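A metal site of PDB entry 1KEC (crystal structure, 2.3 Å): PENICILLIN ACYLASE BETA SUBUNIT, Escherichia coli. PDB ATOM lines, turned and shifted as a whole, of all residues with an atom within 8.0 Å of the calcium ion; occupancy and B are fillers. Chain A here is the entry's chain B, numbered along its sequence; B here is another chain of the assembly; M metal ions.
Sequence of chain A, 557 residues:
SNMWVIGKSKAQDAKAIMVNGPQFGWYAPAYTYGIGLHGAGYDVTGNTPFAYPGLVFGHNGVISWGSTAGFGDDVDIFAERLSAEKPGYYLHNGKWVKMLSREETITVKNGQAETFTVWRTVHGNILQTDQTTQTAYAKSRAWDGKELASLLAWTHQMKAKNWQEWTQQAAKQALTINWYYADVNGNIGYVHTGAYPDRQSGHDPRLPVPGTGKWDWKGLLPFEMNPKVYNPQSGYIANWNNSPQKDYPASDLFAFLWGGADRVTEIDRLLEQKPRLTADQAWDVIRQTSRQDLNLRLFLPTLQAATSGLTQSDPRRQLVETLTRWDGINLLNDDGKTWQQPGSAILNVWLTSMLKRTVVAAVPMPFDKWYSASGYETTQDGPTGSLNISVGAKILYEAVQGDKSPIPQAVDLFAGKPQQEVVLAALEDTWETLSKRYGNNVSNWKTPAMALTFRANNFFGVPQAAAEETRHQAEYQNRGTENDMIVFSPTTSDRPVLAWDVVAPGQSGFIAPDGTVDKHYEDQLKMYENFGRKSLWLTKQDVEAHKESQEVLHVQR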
ATOM      1  N   GLY A  72      27.208 -21.832 -28.971  1.00  0.00           N
ATOM      2  CA  GLY A  72      27.102 -20.843 -30.025  1.00  0.00           C
ATOM      3  C   GLY A  72      27.304 -19.496 -29.323  1.00  0.00           C
ATOM      4  O   GLY A  72      27.345 -19.451 -28.091  1.00  0.00           O
ATOM      5  N   ASP A  73      27.447 -18.413 -30.083  1.00  0.00           N
ATOM      6  CA  ASP A  73      27.624 -17.094 -29.487  1.00  0.00           C
ATOM      7  C   ASP A  73      26.268 -16.396 -29.305  1.00  0.00           C
ATOM      8  O   ASP A  73      25.766 -15.745 -30.220  1.00  0.00           O
ATOM      9  CB  ASP A  73      28.549 -16.240 -30.354  1.00  0.00           C
ATOM     10  CG  ASP A  73      28.894 -14.906 -29.709  1.00  0.00           C
ATOM     11  OD1 ASP A  73      28.292 -14.547 -28.651  1.00  0.00           O
ATOM     12  OD2 ASP A  73      29.769 -14.141 -30.183  1.00  0.00           O
ATOM     13  N   ASP A  74      25.688 -16.508 -28.110  1.00  0.00           N
ATOM     14  CA  ASP A  74      24.397 -15.904 -27.835  1.00  0.00           C
ATOM     15  C   ASP A  74      24.459 -14.797 -26.769  1.00  0.00           C
ATOM     16  O   ASP A  74      23.416 -14.377 -26.244  1.00  0.00           O
ATOM     17  CB  ASP A  74      23.399 -16.978 -27.432  1.00  0.00           C
ATOM     18  CG  ASP A  74      23.850 -17.734 -26.208  1.00  0.00           C
ATOM     19  OD1 ASP A  74      24.998 -17.526 -25.775  1.00  0.00           O
ATOM     20  OD2 ASP A  74      23.119 -18.534 -25.598  1.00  0.00           O
ATOM     21  N   VAL A  75      25.672 -14.311 -26.480  1.00  0.00           N
ATOM     22  CA  VAL A  75      25.911 -13.231 -25.518  1.00  0.00           C
ATOM     23  C   VAL A  75      26.891 -12.167 -26.056  1.00  0.00           C
ATOM     24  O   VAL A  75      28.014 -12.472 -26.471  1.00  0.00           O
ATOM     25  CB  VAL A  75      26.527 -13.789 -24.222  1.00  0.00           C
ATOM     26  CG1 VAL A  75      26.602 -12.665 -23.150  1.00  0.00           C
ATOM     27  CG2 VAL A  75      25.710 -14.944 -23.685  1.00  0.00           C
ATOM     28  N   ASP A  76      26.465 -10.912 -26.049  1.00  0.00           N
ATOM     29  CA  ASP A  76      27.360  -9.831 -26.443  1.00  0.00           C
ATOM     30  C   ASP A  76      27.441  -8.875 -25.260  1.00  0.00           C
ATOM     31  O   ASP A  76      26.557  -8.871 -24.404  1.00  0.00           O
ATOM     32  CB  ASP A  76      26.866  -9.071 -27.683  1.00  0.00           C
ATOM     33  CG  ASP A  76      26.823  -9.918 -28.963  1.00  0.00           C
ATOM     34  OD1 ASP A  76      27.590 -10.921 -29.100  1.00  0.00           O
ATOM     35  OD2 ASP A  76      26.018  -9.626 -29.903  1.00  0.00           O
ATOM     36  N   ILE A  77      28.466  -8.045 -25.242  1.00  0.00           N
ATOM     37  CA  ILE A  77      28.648  -7.099 -24.146  1.00  0.00           C
ATOM     38  C   ILE A  77      28.507  -5.662 -24.614  1.00  0.00           C
ATOM     39  O   ILE A  77      29.153  -5.243 -25.585  1.00  0.00           O
ATOM     40  CB  ILE A  77      30.027  -7.339 -23.519  1.00  0.00           C
ATOM     41  CG1 ILE A  77      30.043  -8.731 -22.868  1.00  0.00           C
ATOM     42  CG2 ILE A  77      30.358  -6.250 -22.526  1.00  0.00           C
ATOM     43  CD1 ILE A  77      31.104  -8.942 -21.831  1.00  0.00           C
ATOM     44  N   SER A 140      24.554  -8.996 -22.381  1.00  0.00           N
ATOM     45  CA  SER A 140      23.351  -9.169 -23.159  1.00  0.00           C
ATOM     46  C   SER A 140      23.160 -10.596 -23.677  1.00  0.00           C
ATOM     47  O   SER A 140      23.897 -11.069 -24.544  1.00  0.00           O
ATOM     48  CB  SER A 140      23.397  -8.198 -24.333  1.00  0.00           C
ATOM     49  OG  SER A 140      22.132  -8.051 -24.921  1.00  0.00           O
ATOM     50  N   PRO A 197      21.170 -13.503 -31.743  1.00  0.00           N
ATOM     51  CA  PRO A 197      20.869 -12.121 -32.115  1.00  0.00           C
ATOM     52  C   PRO A 197      21.107 -11.767 -33.560  1.00  0.00           C
ATOM     53  O   PRO A 197      22.041 -12.259 -34.198  1.00  0.00           O
ATOM     54  CB  PRO A 197      21.802 -11.299 -31.207  1.00  0.00           C
ATOM     55  CG  PRO A 197      22.955 -12.220 -30.914  1.00  0.00           C
ATOM     56  CD  PRO A 197      22.392 -13.602 -30.919  1.00  0.00           C
ATOM     57  N   ARG A 199      22.452  -9.210 -35.499  1.00  0.00           N
ATOM     58  CA  ARG A 199      23.378  -8.130 -35.239  1.00  0.00           C
ATOM     59  C   ARG A 199      23.476  -7.090 -36.358  1.00  0.00           C
ATOM     60  O   ARG A 199      23.296  -7.424 -37.536  1.00  0.00           O
ATOM     61  CB  ARG A 199      24.762  -8.709 -34.944  1.00  0.00           C
ATOM     62  CG  ARG A 199      24.828  -9.655 -33.738  1.00  0.00           C
ATOM     63  CD  ARG A 199      26.254 -10.086 -33.388  1.00  0.00           C
ATOM     64  NE  ARG A 199      26.408 -10.916 -32.186  1.00  0.00           N
ATOM     65  CZ  ARG A 199      26.290 -12.245 -32.126  1.00  0.00           C
ATOM     66  NH1 ARG A 199      25.948 -12.983 -33.192  1.00  0.00           N
ATOM     67  NH2 ARG A 199      26.502 -12.863 -30.971  1.00  0.00           N
ATOM     68  N   HIS A 203      29.174  -5.500 -36.944  1.00  0.00           N
ATOM     69  CA  HIS A 203      29.314  -5.899 -35.550  1.00  0.00           C
ATOM     70  C   HIS A 203      30.119  -7.192 -35.447  1.00  0.00           C
ATOM     71  O   HIS A 203      29.640  -8.259 -35.788  1.00  0.00           O
ATOM     72  CB  HIS A 203      27.905  -6.077 -34.939  1.00  0.00           C
ATOM     73  CG  HIS A 203      27.897  -6.569 -33.524  1.00  0.00           C
ATOM     74  ND1 HIS A 203      26.796  -6.424 -32.715  1.00  0.00           N
ATOM     75  CD2 HIS A 203      28.837  -7.209 -32.791  1.00  0.00           C
ATOM     76  CE1 HIS A 203      27.060  -6.953 -31.528  1.00  0.00           C
ATOM     77  NE2 HIS A 203      28.278  -7.444 -31.551  1.00  0.00           N
ATOM     78  N   ASP A 204      31.340  -7.083 -34.956  1.00  0.00           N
ATOM     79  CA  ASP A 204      32.225  -8.218 -34.745  1.00  0.00           C
ATOM     80  C   ASP A 204      31.798  -8.795 -33.400  1.00  0.00           C
ATOM     81  O   ASP A 204      32.075  -8.216 -32.348  1.00  0.00           O
ATOM     82  CB  ASP A 204      33.658  -7.707 -34.690  1.00  0.00           C
ATOM     83  CG  ASP A 204      34.702  -8.801 -34.603  1.00  0.00           C
ATOM     84  OD1 ASP A 204      34.496  -9.865 -33.919  1.00  0.00           O
ATOM     85  OD2 ASP A 204      35.812  -8.650 -35.169  1.00  0.00           O
ATOM     86  N   PRO A 205      31.198  -9.973 -33.427  1.00  0.00           N
ATOM     87  CA  PRO A 205      30.590 -10.576 -32.229  1.00  0.00           C
ATOM     88  C   PRO A 205      31.606 -11.079 -31.189  1.00  0.00           C
ATOM     89  O   PRO A 205      31.213 -11.643 -30.177  1.00  0.00           O
ATOM     90  CB  PRO A 205      29.796 -11.763 -32.789  1.00  0.00           C
ATOM     91  CG  PRO A 205      30.505 -12.139 -34.075  1.00  0.00           C
ATOM     92  CD  PRO A 205      31.170 -10.864 -34.612  1.00  0.00           C
ATOM     93  N   ARG A 206      32.896 -10.894 -31.445  1.00  0.00           N
ATOM     94  CA  ARG A 206      33.923 -11.343 -30.521  1.00  0.00           C
ATOM     95  C   ARG A 206      34.363 -10.181 -29.642  1.00  0.00           C
ATOM     96  O   ARG A 206      35.129 -10.352 -28.705  1.00  0.00           O
ATOM     97  CB  ARG A 206      35.143 -11.839 -31.296  1.00  0.00           C
ATOM     98  CG  ARG A 206      34.874 -12.961 -32.270  1.00  0.00           C
ATOM     99  CD  ARG A 206      36.014 -13.213 -33.220  1.00  0.00           C
ATOM    100  NE  ARG A 206      36.283 -12.040 -34.036  1.00  0.00           N
ATOM    101  CZ  ARG A 206      37.279 -11.969 -34.913  1.00  0.00           C
ATOM    102  NH1 ARG A 206      38.093 -13.011 -35.060  1.00  0.00           N
ATOM    103  NH2 ARG A 206      37.496 -10.857 -35.607  1.00  0.00           N
ATOM    104  N   LEU A 207      33.874  -8.994 -29.959  1.00  0.00           N
ATOM    105  CA  LEU A 207      34.329  -7.805 -29.272  1.00  0.00           C
ATOM    106  C   LEU A 207      33.118  -7.006 -28.786  1.00  0.00           C
ATOM    107  O   LEU A 207      32.044  -7.140 -29.355  1.00  0.00           O
ATOM    108  CB  LEU A 207      35.212  -7.003 -30.237  1.00  0.00           C
ATOM    109  CG  LEU A 207      36.400  -7.876 -30.655  1.00  0.00           C
ATOM    110  CD1 LEU A 207      37.183  -7.325 -31.828  1.00  0.00           C
ATOM    111  CD2 LEU A 207      37.345  -8.068 -29.461  1.00  0.00           C
ATOM    112  N   PRO A 208      33.277  -6.213 -27.739  1.00  0.00           N
ATOM    113  CA  PRO A 208      32.157  -5.444 -27.190  1.00  0.00           C
ATOM    114  C   PRO A 208      31.647  -4.366 -28.161  1.00  0.00           C
ATOM    115  O   PRO A 208      32.342  -3.996 -29.106  1.00  0.00           O
ATOM    116  CB  PRO A 208      32.739  -4.775 -25.932  1.00  0.00           C
ATOM    117  CG  PRO A 208      34.066  -5.472 -25.661  1.00  0.00           C
ATOM    118  CD  PRO A 208      34.528  -6.016 -26.982  1.00  0.00           C
ATOM    119  N   TRP A 217      21.072  -4.772 -31.007  1.00  0.00           N
ATOM    120  CA  TRP A 217      20.675  -5.874 -31.868  1.00  0.00           C
ATOM    121  C   TRP A 217      19.399  -5.495 -32.613  1.00  0.00           C
ATOM    122  O   TRP A 217      18.577  -4.741 -32.093  1.00  0.00           O
ATOM    123  CB  TRP A 217      20.358  -7.091 -31.022  1.00  0.00           C
ATOM    124  CG  TRP A 217      21.527  -7.732 -30.336  1.00  0.00           C
ATOM    125  CD1 TRP A 217      22.839  -7.577 -30.631  1.00  0.00           C
ATOM    126  CD2 TRP A 217      21.453  -8.676 -29.278  1.00  0.00           C
ATOM    127  NE1 TRP A 217      23.603  -8.372 -29.802  1.00  0.00           N
ATOM    128  CE2 TRP A 217      22.767  -9.048 -28.964  1.00  0.00           C
ATOM    129  CE3 TRP A 217      20.393  -9.266 -28.575  1.00  0.00           C
ATOM    130  CZ2 TRP A 217      23.060  -9.970 -27.970  1.00  0.00           C
ATOM    131  CZ3 TRP A 217      20.682 -10.176 -27.575  1.00  0.00           C
ATOM    132  CH2 TRP A 217      22.011 -10.510 -27.277  1.00  0.00           C
ATOM    133  N   ALA A 250      31.455 -19.937 -33.538  1.00  0.00           N
ATOM    134  CA  ALA A 250      31.422 -20.380 -32.170  1.00  0.00           C
ATOM    135  C   ALA A 250      31.279 -19.265 -31.156  1.00  0.00           C
ATOM    136  O   ALA A 250      31.363 -18.074 -31.464  1.00  0.00           O
ATOM    137  CB  ALA A 250      32.676 -21.167 -31.861  1.00  0.00           C
ATOM    138  N   SER A 251      31.082 -19.708 -29.930  1.00  0.00           N
ATOM    139  CA  SER A 251      31.127 -18.886 -28.712  1.00  0.00           C
ATOM    140  C   SER A 251      32.326 -17.942 -28.758  1.00  0.00           C
ATOM    141  O   SER A 251      33.382 -18.323 -29.270  1.00  0.00           O
ATOM    142  CB  SER A 251      31.329 -19.841 -27.542  1.00  0.00           C
ATOM    143  OG  SER A 251      31.686 -19.127 -26.389  1.00  0.00           O
ATOM    144  N   ASP A 252      32.178 -16.721 -28.233  1.00  0.00           N
ATOM    145  CA  ASP A 252      33.297 -15.756 -28.220  1.00  0.00           C
ATOM    146  C   ASP A 252      34.443 -16.032 -27.232  1.00  0.00           C
ATOM    147  O   ASP A 252      35.465 -15.342 -27.261  1.00  0.00           O
ATOM    148  CB  ASP A 252      32.823 -14.288 -28.143  1.00  0.00           C
ATOM    149  CG  ASP A 252      32.114 -13.953 -26.854  1.00  0.00           C
ATOM    150  OD1 ASP A 252      32.632 -14.304 -25.782  1.00  0.00           O
ATOM    151  OD2 ASP A 252      31.027 -13.329 -26.827  1.00  0.00           O
ATOM    152  N   LEU A 253      34.314 -17.041 -26.384  1.00  0.00           N
ATOM    153  CA  LEU A 253      35.367 -17.391 -25.417  1.00  0.00           C
ATOM    154  C   LEU A 253      36.722 -17.559 -26.086  1.00  0.00           C
ATOM    155  O   LEU A 253      36.858 -18.368 -27.000  1.00  0.00           O
ATOM    156  CB  LEU A 253      35.023 -18.679 -24.674  1.00  0.00           C
ATOM    157  CG  LEU A 253      33.787 -18.703 -23.782  1.00  0.00           C
ATOM    158  CD1 LEU A 253      33.485 -20.123 -23.256  1.00  0.00           C
ATOM    159  CD2 LEU A 253      33.934 -17.698 -22.628  1.00  0.00           C
ATOM    160  N   SER B 150      28.124 -17.676 -21.527  1.00  0.00           N
ATOM    161  CA  SER B 150      29.557 -17.509 -21.747  1.00  0.00           C
ATOM    162  C   SER B 150      29.986 -16.424 -22.721  1.00  0.00           C
ATOM    163  O   SER B 150      29.535 -16.401 -23.883  1.00  0.00           O
ATOM    164  CB  SER B 150      30.144 -18.826 -22.254  1.00  0.00           C
ATOM    165  OG  SER B 150      30.088 -19.790 -21.229  1.00  0.00           O
ATOM    166  N   THR B 151      30.885 -15.548 -22.264  1.00  0.00           N
ATOM    167  CA  THR B 151      31.474 -14.515 -23.108  1.00  0.00           C
ATOM    168  C   THR B 151      32.777 -14.035 -22.481  1.00  0.00           C
ATOM    169  O   THR B 151      32.908 -14.077 -21.267  1.00  0.00           O
ATOM    170  CB  THR B 151      30.522 -13.311 -23.283  1.00  0.00           C
ATOM    171  OG1 THR B 151      31.028 -12.438 -24.310  1.00  0.00           O
ATOM    172  CG2 THR B 151      30.530 -12.420 -22.028  1.00  0.00           C
ATOM    173  N   SER B 152      33.736 -13.616 -23.290  1.00  0.00           N
ATOM    174  CA  SER B 152      34.991 -13.040 -22.799  1.00  0.00           C
ATOM    175  C   SER B 152      35.374 -11.860 -23.696  1.00  0.00           C
ATOM    176  O   SER B 152      36.552 -11.590 -23.940  1.00  0.00           O
ATOM    177  CB  SER B 152      36.109 -14.089 -22.776  1.00  0.00           C
ATOM    178  OG  SER B 152      36.504 -14.522 -24.079  1.00  0.00           O
ATOM    179  N   GLU B 153      34.355 -11.169 -24.202  1.00  0.00           N
ATOM    180  CA  GLU B 153      34.564 -10.054 -25.117  1.00  0.00           C
ATOM    181  C   GLU B 153      35.510  -8.987 -24.543  1.00  0.00           C
ATOM    182  O   GLU B 153      36.364  -8.450 -25.258  1.00  0.00           O
ATOM    183  CB  GLU B 153      33.234  -9.437 -25.539  1.00  0.00           C
ATOM    184  CG  GLU B 153      32.475 -10.275 -26.559  1.00  0.00           C
ATOM    185  CD  GLU B 153      31.139  -9.665 -26.939  1.00  0.00           C
ATOM    186  OE1 GLU B 153      30.940  -8.478 -26.634  1.00  0.00           O
ATOM    187  OE2 GLU B 153      30.291 -10.385 -27.531  1.00  0.00           O
ATOM    188  N   ASN B 156      38.868 -10.370 -24.779  1.00  0.00           N
ATOM    189  CA  ASN B 156      39.188 -10.408 -26.196  1.00  0.00           C
ATOM    190  C   ASN B 156      39.700  -9.053 -26.716  1.00  0.00           C
ATOM    191  O   ASN B 156      40.718  -8.992 -27.414  1.00  0.00           O
ATOM    192  CB  ASN B 156      37.971 -10.875 -27.012  1.00  0.00           C
ATOM    193  CG  ASN B 156      37.494 -12.279 -26.601  1.00  0.00           C
ATOM    194  OD1 ASN B 156      38.216 -13.035 -25.954  1.00  0.00           O
ATOM    195  ND2 ASN B 156      36.263 -12.626 -26.999  1.00  0.00           N
HETATM  196 CA    CA M   1      29.565 -12.282 -28.375  1.00  0.00          CA
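The calcium ion is bound by OE2 of Glu 153 of chain B (2.2 Å), OD2 of Asp 252 (2.4 Å), O of Val 75 (2.5 Å), OD1 of Asp 76 (2.5 Å), O of Pro 205 (2.5 Å), OD2 of Asp 73 (2.6 Å) and OD1 of Asp 73 (2.6 Å).
The side-chain carboxylate (OE1) of Glu 153 of chain B lies within hydrogen-bond range of the backbone NH (N) of Ile 77 (2.9 Å).
The backbone carbonyl oxygen (O) of Asp 73 is in hydrogen-bond range of the guanidinium group (NH2) of Arg 199 (3.1 Å).
NE of Arg 199 is in salt-bridge range of OD2 of Asp 76.
OD2 of Asp 76 is in hydrogen-bond range of NE1 of Trp 217, at 2.7 Å.
The side-chain carboxylate (OD1) of Asp 252 sits at hydrogen-bond distance from the backbone NH (N) of Ser 152 of chain B (2.8 Å).
The backbone NH (N) of Ser 140 sits at hydrogen-bond distance from the backbone carbonyl oxygen (O) of Asp 76, 2.8 Å away.
The side-chain carboxylate (OD1) of Asp 252 lies within hydrogen-bond range of the side-chain hydroxyl (OG1) of Thr 151 of chain B, 2.9 Å away.
ND2 of Asn 156 of chain B lies within hydrogen-bond range of O of Asp 252 (2.8 Å).
Six residues have an atom within 4 Å of the calcium ion: Asp 73, Val 75, Asp 76, Pro 205, Asp 252 and Glu 153 of chain B.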
